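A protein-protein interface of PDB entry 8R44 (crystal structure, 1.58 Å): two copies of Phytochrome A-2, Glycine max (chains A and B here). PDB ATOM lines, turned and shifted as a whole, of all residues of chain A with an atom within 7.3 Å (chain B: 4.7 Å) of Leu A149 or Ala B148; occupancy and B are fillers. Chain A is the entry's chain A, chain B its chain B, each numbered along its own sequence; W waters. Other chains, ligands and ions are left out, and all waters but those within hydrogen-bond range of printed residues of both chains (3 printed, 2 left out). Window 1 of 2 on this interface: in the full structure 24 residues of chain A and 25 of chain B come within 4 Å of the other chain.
The side-chain hydroxyl (OH) of Tyr B334 sits at hydrogen-bond distance from the side-chain amino group (NZ) of Lys A153.
Among the printed residues, pairs that only touch across the chains: Ala A145 with Thr B144, Lys A153 with Tyr B152, Thr A144 with Thr B144, Ala A146 with Pro B106, Ala A146 with Asn B105, Leu A149 with Asn B105, Leu A149 with Ala B148, Leu A149 with Pro B106, Ala A148 with Leu B149, Tyr A152 with Tyr B152, Tyr A152 with Leu B149, Leu A149 with Tyr B152 and Leu A149 with Tyr B334.
Of the printed residues of chain B, Ala A145 touches Thr B144 (3.1 Å).
Printed residues of chain B within 4 Å of Leu A149: Asn B105, Pro B106, Ala B148, Tyr B152 and Tyr B334.
Of the printed residues of chain B, Tyr A152 touches Leu B149 (3.8 Å) and Tyr B152 (3.8 Å).
Printed residues of chain A within 4 Å of Thr B144: Thr A144 and Ala A145.
No residue of chain A comes within 4 Å of Gly B147.
Of chain A, only Leu A149 (3.7 Å) comes within 4 Å of Ala B148.
The nearest residue of chain B that does not touch Leu A149 is Pro B331 (4.1 Å).
The nearest printed residue of chain A that does not touch Asn B105 is Ala A145 (4.9 Å).
Of the 14 printed residues of chain B, 7 touch a printed residue of chain A.
Of the 14 printed residues of chain A, 7 touch a printed residue of chain B.
Among the printed residues, 14 pairs touch across the chains.
Among the printed residues, no Asp or Glu carboxylate lies within 4 Å of a Lys or Arg side-chain nitrogen of the other chain.
Thr A144 touches its own counterpart, Thr B144.
Ala A145 touches Thr B144, but with the chains exchanged Thr A144 does not touch Ala B145 (4.3 Å).
Leu A149 touches Tyr B152, and with the chains exchanged Tyr A152 touches Leu B149.
Tyr A152 touches its own counterpart, Tyr B152.
Positions printed for both chains: 144, 145, 146, 147, 148, 149, 150, 151, 152 and 331.
Of the 14 pairs that touch across the chains among the printed residues, 6 have their exchanged pair printed and touching as well.
Water W1 lies within hydrogen-bond range of OH of Tyr B334 (2.6 Å) and OE1 of Gln A150 (2.7 Å).
Water W3 bridges the backbone carbonyl oxygen (O) of Ala A146 (2.8 Å) and the backbone carbonyl oxygen (O) of Asn B105 (2.8 Å).
Water W2 lies within hydrogen-bond range of the side-chain hydroxyl of Thr B144 (2.9 Å), the side-chain hydroxyl of Thr A144 (2.9 Å) and the backbone NH of Ala A145 (3.0 Å).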
ATOM      1  N   MET A 143       8.129   7.179  25.021  1.00  0.00           N
ATOM      2  CA  MET A 143       9.073   7.902  25.840  1.00  0.00           C
ATOM      3  C   MET A 143      10.130   6.979  26.477  1.00  0.00           C
ATOM      4  O   MET A 143      10.860   7.409  27.374  1.00  0.00           O
ATOM      5  CB  MET A 143       8.311   8.627  26.952  1.00  0.00           C
ATOM      6  CG  MET A 143       7.232   9.561  26.445  1.00  0.00           C
ATOM      7  SD  MET A 143       7.861  10.797  25.316  1.00  0.00           S
ATOM      8  CE  MET A 143       8.971  11.775  26.345  1.00  0.00           C
ATOM      9  N   THR A 144      10.301   5.729  26.014  1.00  0.00           N
ATOM     10  CA  THR A 144      11.179   4.817  26.725  1.00  0.00           C
ATOM     11  C   THR A 144      12.644   5.288  26.653  1.00  0.00           C
ATOM     12  O   THR A 144      13.330   5.306  27.673  1.00  0.00           O
ATOM     13  CB  THR A 144      10.996   3.367  26.254  1.00  0.00           C
ATOM     14  OG1 THR A 144      11.195   3.314  24.871  1.00  0.00           O
ATOM     15  CG2 THR A 144       9.618   2.835  26.455  1.00  0.00           C
ATOM     16  N   ALA A 145      13.141   5.635  25.452  1.00  0.00           N
ATOM     17  CA  ALA A 145      14.501   6.139  25.344  1.00  0.00           C
ATOM     18  C   ALA A 145      14.660   7.422  26.153  1.00  0.00           C
ATOM     19  O   ALA A 145      15.691   7.663  26.781  1.00  0.00           O
ATOM     20  CB  ALA A 145      14.926   6.372  23.896  1.00  0.00           C
ATOM     21  N   ALA A 146      13.701   8.348  26.030  1.00  0.00           N
ATOM     22  CA  ALA A 146      13.752   9.607  26.752  1.00  0.00           C
ATOM     23  C   ALA A 146      13.918   9.363  28.241  1.00  0.00           C
ATOM     24  O   ALA A 146      14.723  10.049  28.871  1.00  0.00           O
ATOM     25  CB  ALA A 146      12.486  10.427  26.472  1.00  0.00           C
ATOM     26  N   GLY A 147      13.075   8.474  28.782  1.00  0.00           N
ATOM     27  CA  GLY A 147      13.145   8.162  30.202  1.00  0.00           C
ATOM     28  C   GLY A 147      14.477   7.532  30.609  1.00  0.00           C
ATOM     29  O   GLY A 147      15.014   7.820  31.685  1.00  0.00           O
ATOM     30  N   ALA A 148      15.017   6.653  29.759  1.00  0.00           N
ATOM     31  CA  ALA A 148      16.309   6.029  30.016  1.00  0.00           C
ATOM     32  C   ALA A 148      17.463   7.045  30.028  1.00  0.00           C
ATOM     33  O   ALA A 148      18.287   7.038  30.951  1.00  0.00           O
ATOM     34  CB  ALA A 148      16.525   4.914  29.012  1.00  0.00           C
ATOM     35  N   LEU A 149      17.478   7.942  29.042  1.00  0.00           N
ATOM     36  CA  LEU A 149      18.453   9.022  29.023  1.00  0.00           C
ATOM     37  C   LEU A 149      18.336   9.887  30.276  1.00  0.00           C
ATOM     38  O   LEU A 149      19.346  10.225  30.871  1.00  0.00           O
ATOM     39  CB  LEU A 149      18.297   9.871  27.764  1.00  0.00           C
ATOM     40  CG  LEU A 149      18.614   9.155  26.451  1.00  0.00           C
ATOM     41  CD1 LEU A 149      18.141   9.962  25.277  1.00  0.00           C
ATOM     42  CD2 LEU A 149      20.105   8.829  26.346  1.00  0.00           C
ATOM     43  N   GLN A 150      17.107  10.222  30.683  1.00  0.00           N
ATOM     44  CA  GLN A 150      16.960  11.124  31.826  1.00  0.00           C
ATOM     45  C   GLN A 150      17.432  10.418  33.104  1.00  0.00           C
ATOM     46  O   GLN A 150      18.055  11.053  33.958  1.00  0.00           O
ATOM     47  CB  GLN A 150      15.520  11.625  31.867  1.00  0.00           C
ATOM     48  CG  GLN A 150      15.190  12.417  33.106  1.00  0.00           C
ATOM     49  CD  GLN A 150      15.745  13.811  33.073  1.00  0.00           C
ATOM     50  OE1 GLN A 150      16.475  14.239  32.170  1.00  0.00           O
ATOM     51  NE2 GLN A 150      15.407  14.561  34.115  1.00  0.00           N
ATOM     52  N   SER A 151      17.155   9.116  33.253  1.00  0.00           N
ATOM     53  CA  SER A 151      17.580   8.363  34.424  1.00  0.00           C
ATOM     54  C   SER A 151      19.110   8.402  34.492  1.00  0.00           C
ATOM     55  O   SER A 151      19.683   8.668  35.547  1.00  0.00           O
ATOM     56  CB  SER A 151      17.041   6.941  34.418  1.00  0.00           C
ATOM     57  OG  SER A 151      15.609   6.953  34.499  1.00  0.00           O
ATOM     58  N   TYR A 152      19.776   8.139  33.355  1.00  0.00           N
ATOM     59  CA  TYR A 152      21.243   8.078  33.366  1.00  0.00           C
ATOM     60  C   TYR A 152      21.855   9.460  33.526  1.00  0.00           C
ATOM     61  O   TYR A 152      22.874   9.618  34.219  1.00  0.00           O
ATOM     62  CB  TYR A 152      21.767   7.314  32.156  1.00  0.00           C
ATOM     63  CG  TYR A 152      22.886   6.371  32.492  1.00  0.00           C
ATOM     64  CD1 TYR A 152      24.130   6.838  32.847  1.00  0.00           C
ATOM     65  CD2 TYR A 152      22.676   4.995  32.498  1.00  0.00           C
ATOM     66  CE1 TYR A 152      25.151   5.970  33.225  1.00  0.00           C
ATOM     67  CE2 TYR A 152      23.688   4.120  32.846  1.00  0.00           C
ATOM     68  CZ  TYR A 152      24.917   4.609  33.247  1.00  0.00           C
ATOM     69  OH  TYR A 152      25.935   3.744  33.619  1.00  0.00           O
ATOM     70  N   LYS A 153      21.245  10.473  32.893  1.00  0.00           N
ATOM     71  CA  LYS A 153      21.690  11.845  33.051  1.00  0.00           C
ATOM     72  C   LYS A 153      21.657  12.232  34.523  1.00  0.00           C
ATOM     73  O   LYS A 153      22.629  12.829  35.019  1.00  0.00           O
ATOM     74  CB  LYS A 153      20.828  12.809  32.227  1.00  0.00           C
ATOM     75  CG  LYS A 153      21.200  14.278  32.376  1.00  0.00           C
ATOM     76  CD  LYS A 153      20.341  15.135  31.446  1.00  0.00           C
ATOM     77  CE  LYS A 153      20.576  16.618  31.606  1.00  0.00           C
ATOM     78  NZ  LYS A 153      19.820  17.403  30.585  1.00  0.00           N
ATOM     79  N   LEU A 154      20.544  11.951  35.216  1.00  0.00           N
ATOM     80  CA  LEU A 154      20.454  12.310  36.629  1.00  0.00           C
ATOM     81  C   LEU A 154      21.535  11.594  37.445  1.00  0.00           C
ATOM     82  O   LEU A 154      22.181  12.207  38.295  1.00  0.00           O
ATOM     83  CB  LEU A 154      19.048  12.039  37.168  1.00  0.00           C
ATOM     84  CG  LEU A 154      17.953  12.938  36.599  1.00  0.00           C
ATOM     85  CD1 LEU A 154      16.576  12.418  36.941  1.00  0.00           C
ATOM     86  CD2 LEU A 154      18.133  14.361  37.051  1.00  0.00           C
ATOM     87  N   ALA A 155      21.779  10.310  37.152  1.00  0.00           N
ATOM     88  CA  ALA A 155      22.817   9.557  37.845  1.00  0.00           C
ATOM     89  C   ALA A 155      24.215  10.103  37.547  1.00  0.00           C
ATOM     90  O   ALA A 155      25.070  10.195  38.445  1.00  0.00           O
ATOM     91  CB  ALA A 155      22.736   8.100  37.476  1.00  0.00           C
ATOM     92  N   PRO A 331      15.547   0.896  33.714  1.00  0.00           N
ATOM     93  CA  PRO A 331      16.571   1.864  33.349  1.00  0.00           C
ATOM     94  C   PRO A 331      17.066   2.685  34.541  1.00  0.00           C
ATOM     95  O   PRO A 331      18.256   2.988  34.580  1.00  0.00           O
ATOM     96  CB  PRO A 331      15.905   2.731  32.259  1.00  0.00           C
ATOM     97  CG  PRO A 331      14.938   1.755  31.644  1.00  0.00           C
ATOM     98  CD  PRO A 331      14.375   0.999  32.837  1.00  0.00           C
ATOM     99  N   ASN B 105      13.786  14.384  25.539  1.00  0.00           N
ATOM    100  CA  ASN B 105      13.911  13.914  24.159  1.00  0.00           C
ATOM    101  C   ASN B 105      14.691  12.608  24.149  1.00  0.00           C
ATOM    102  O   ASN B 105      15.425  12.303  25.105  1.00  0.00           O
ATOM    103  CB  ASN B 105      14.640  14.949  23.317  1.00  0.00           C
ATOM    104  CG  ASN B 105      13.702  16.023  22.808  1.00  0.00           C
ATOM    105  OD1 ASN B 105      12.633  15.720  22.271  1.00  0.00           O
ATOM    106  ND2 ASN B 105      14.095  17.286  22.987  1.00  0.00           N
ATOM    107  N   PRO B 106      14.619  11.826  23.052  1.00  0.00           N
ATOM    108  CA  PRO B 106      13.682  12.008  21.937  1.00  0.00           C
ATOM    109  C   PRO B 106      12.398  11.225  22.196  1.00  0.00           C
ATOM    110  O   PRO B 106      12.401  10.358  23.050  1.00  0.00           O
ATOM    111  CB  PRO B 106      14.424  11.312  20.775  1.00  0.00           C
ATOM    112  CG  PRO B 106      15.135  10.137  21.459  1.00  0.00           C
ATOM    113  CD  PRO B 106      15.422  10.604  22.887  1.00  0.00           C
ATOM    114  N   THR B 144      15.693   0.567  21.847  1.00  0.00           N
ATOM    115  CA  THR B 144      15.824   2.014  22.037  1.00  0.00           C
ATOM    116  C   THR B 144      16.304   2.395  23.443  1.00  0.00           C
ATOM    117  O   THR B 144      17.229   3.200  23.570  1.00  0.00           O
ATOM    118  CB  THR B 144      14.511   2.720  21.674  1.00  0.00           C
ATOM    119  OG1 THR B 144      14.589   4.092  21.881  1.00  0.00           O
ATOM    120  CG2 THR B 144      13.324   2.308  22.473  1.00  0.00           C
ATOM    121  N   ALA B 145      15.750   1.760  24.468  1.00  0.00           N
ATOM    122  CA  ALA B 145      16.184   2.067  25.830  1.00  0.00           C
ATOM    123  C   ALA B 145      17.563   1.495  26.052  1.00  0.00           C
ATOM    124  O   ALA B 145      18.433   2.129  26.634  1.00  0.00           O
ATOM    125  CB  ALA B 145      15.189   1.540  26.849  1.00  0.00           C
ATOM    126  N   ALA B 146      17.813   0.271  25.536  1.00  0.00           N
ATOM    127  CA  ALA B 146      19.098  -0.365  25.741  1.00  0.00           C
ATOM    128  C   ALA B 146      20.212   0.520  25.180  1.00  0.00           C
ATOM    129  O   ALA B 146      21.287   0.635  25.771  1.00  0.00           O
ATOM    130  CB  ALA B 146      19.106  -1.740  25.088  1.00  0.00           C
ATOM    131  N   GLY B 147      20.026   0.965  23.932  1.00  0.00           N
ATOM    132  CA  GLY B 147      21.032   1.751  23.222  1.00  0.00           C
ATOM    133  C   GLY B 147      21.270   3.119  23.872  1.00  0.00           C
ATOM    134  O   GLY B 147      22.389   3.602  23.921  1.00  0.00           O
ATOM    135  N   ALA B 148      20.192   3.720  24.371  1.00  0.00           N
ATOM    136  CA  ALA B 148      20.276   4.971  25.110  1.00  0.00           C
ATOM    137  C   ALA B 148      21.081   4.802  26.392  1.00  0.00           C
ATOM    138  O   ALA B 148      22.005   5.581  26.634  1.00  0.00           O
ATOM    139  CB  ALA B 148      18.898   5.523  25.372  1.00  0.00           C
ATOM    140  N   LEU B 149      20.797   3.770  27.192  1.00  0.00           N
ATOM    141  CA  LEU B 149      21.588   3.522  28.383  1.00  0.00           C
ATOM    142  C   LEU B 149      23.052   3.277  28.048  1.00  0.00           C
ATOM    143  O   LEU B 149      23.947   3.699  28.750  1.00  0.00           O
ATOM    144  CB  LEU B 149      21.002   2.342  29.143  1.00  0.00           C
ATOM    145  CG  LEU B 149      19.591   2.531  29.678  1.00  0.00           C
ATOM    146  CD1 LEU B 149      19.011   1.211  30.144  1.00  0.00           C
ATOM    147  CD2 LEU B 149      19.583   3.563  30.828  1.00  0.00           C
ATOM    148  N   GLN B 150      23.317   2.495  26.998  1.00  0.00           N
ATOM    149  CA  GLN B 150      24.693   2.162  26.672  1.00  0.00           C
ATOM    150  C   GLN B 150      25.443   3.405  26.251  1.00  0.00           C
ATOM    151  O   GLN B 150      26.584   3.560  26.667  1.00  0.00           O
ATOM    152  CB  GLN B 150      24.710   1.065  25.596  1.00  0.00           C
ATOM    153  CG  GLN B 150      26.102   0.687  25.102  1.00  0.00           C
ATOM    154  CD  GLN B 150      26.945  -0.061  26.118  1.00  0.00           C
ATOM    155  OE1 GLN B 150      26.558  -0.342  27.264  1.00  0.00           O
ATOM    156  NE2 GLN B 150      28.184  -0.303  25.713  1.00  0.00           N
ATOM    157  N   SER B 151      24.818   4.266  25.423  1.00  0.00           N
ATOM    158  CA  SER B 151      25.474   5.493  25.021  1.00  0.00           C
ATOM    159  C   SER B 151      25.835   6.383  26.218  1.00  0.00           C
ATOM    160  O   SER B 151      26.943   6.949  26.354  1.00  0.00           O
ATOM    161  CB  SER B 151      24.609   6.242  24.037  1.00  0.00           C
ATOM    162  OG  SER B 151      24.485   5.539  22.827  1.00  0.00           O
ATOM    163  N   TYR B 152      24.873   6.527  27.146  1.00  0.00           N
ATOM    164  CA  TYR B 152      25.124   7.365  28.318  1.00  0.00           C
ATOM    165  C   TYR B 152      26.130   6.727  29.268  1.00  0.00           C
ATOM    166  O   TYR B 152      26.978   7.413  29.842  1.00  0.00           O
ATOM    167  CB  TYR B 152      23.805   7.720  29.016  1.00  0.00           C
ATOM    168  CG  TYR B 152      23.695   9.171  29.403  1.00  0.00           C
ATOM    169  CD1 TYR B 152      24.474   9.713  30.415  1.00  0.00           C
ATOM    170  CD2 TYR B 152      22.905  10.034  28.680  1.00  0.00           C
ATOM    171  CE1 TYR B 152      24.467  11.066  30.688  1.00  0.00           C
ATOM    172  CE2 TYR B 152      22.822  11.377  29.003  1.00  0.00           C
ATOM    173  CZ  TYR B 152      23.605  11.903  30.010  1.00  0.00           C
ATOM    174  OH  TYR B 152      23.561  13.255  30.336  1.00  0.00           O
ATOM    175  N   PHE B 330      20.341  10.508  17.858  1.00  0.00           N
ATOM    176  CA  PHE B 330      20.177  11.531  18.859  1.00  0.00           C
ATOM    177  C   PHE B 330      20.654  11.064  20.238  1.00  0.00           C
ATOM    178  O   PHE B 330      21.312  11.814  20.950  1.00  0.00           O
ATOM    179  CB  PHE B 330      18.734  12.042  18.889  1.00  0.00           C
ATOM    180  CG  PHE B 330      18.517  13.008  20.010  1.00  0.00           C
ATOM    181  CD1 PHE B 330      18.886  14.336  19.860  1.00  0.00           C
ATOM    182  CD2 PHE B 330      18.000  12.594  21.224  1.00  0.00           C
ATOM    183  CE1 PHE B 330      18.788  15.218  20.927  1.00  0.00           C
ATOM    184  CE2 PHE B 330      17.903  13.482  22.297  1.00  0.00           C
ATOM    185  CZ  PHE B 330      18.266  14.801  22.135  1.00  0.00           C
ATOM    186  N   PRO B 331      20.329   9.854  20.726  1.00  0.00           N
ATOM    187  CA  PRO B 331      20.750   9.502  22.090  1.00  0.00           C
ATOM    188  C   PRO B 331      22.253   9.625  22.340  1.00  0.00           C
ATOM    189  O   PRO B 331      22.659  10.110  23.378  1.00  0.00           O
ATOM    190  CB  PRO B 331      20.224   8.064  22.259  1.00  0.00           C
ATOM    191  CG  PRO B 331      18.967   8.074  21.407  1.00  0.00           C
ATOM    192  CD  PRO B 331      19.396   8.853  20.164  1.00  0.00           C
ATOM    193  N   TYR B 334      23.075  13.329  22.517  1.00  0.00           N
ATOM    194  CA  TYR B 334      22.655  13.816  23.822  1.00  0.00           C
ATOM    195  C   TYR B 334      23.673  13.477  24.913  1.00  0.00           C
ATOM    196  O   TYR B 334      23.986  14.346  25.742  1.00  0.00           O
ATOM    197  CB  TYR B 334      21.260  13.248  24.106  1.00  0.00           C
ATOM    198  CG  TYR B 334      20.533  13.868  25.268  1.00  0.00           C
ATOM    199  CD1 TYR B 334      20.216  15.220  25.264  1.00  0.00           C
ATOM    200  CD2 TYR B 334      20.205  13.130  26.394  1.00  0.00           C
ATOM    201  CE1 TYR B 334      19.544  15.807  26.326  1.00  0.00           C
ATOM    202  CE2 TYR B 334      19.556  13.695  27.466  1.00  0.00           C
ATOM    203  CZ  TYR B 334      19.205  15.050  27.447  1.00  0.00           C
ATOM    204  OH  TYR B 334      18.466  15.610  28.498  1.00  0.00           O
HETATM  205  O   HOH W   1      17.200  13.684  29.652  1.00  0.00           O
HETATM  206  O   HOH W   2      12.025   5.079  22.694  1.00  0.00           O
HETATM  207  O   HOH W   3      15.416  12.566  27.911  1.00  0.00           O
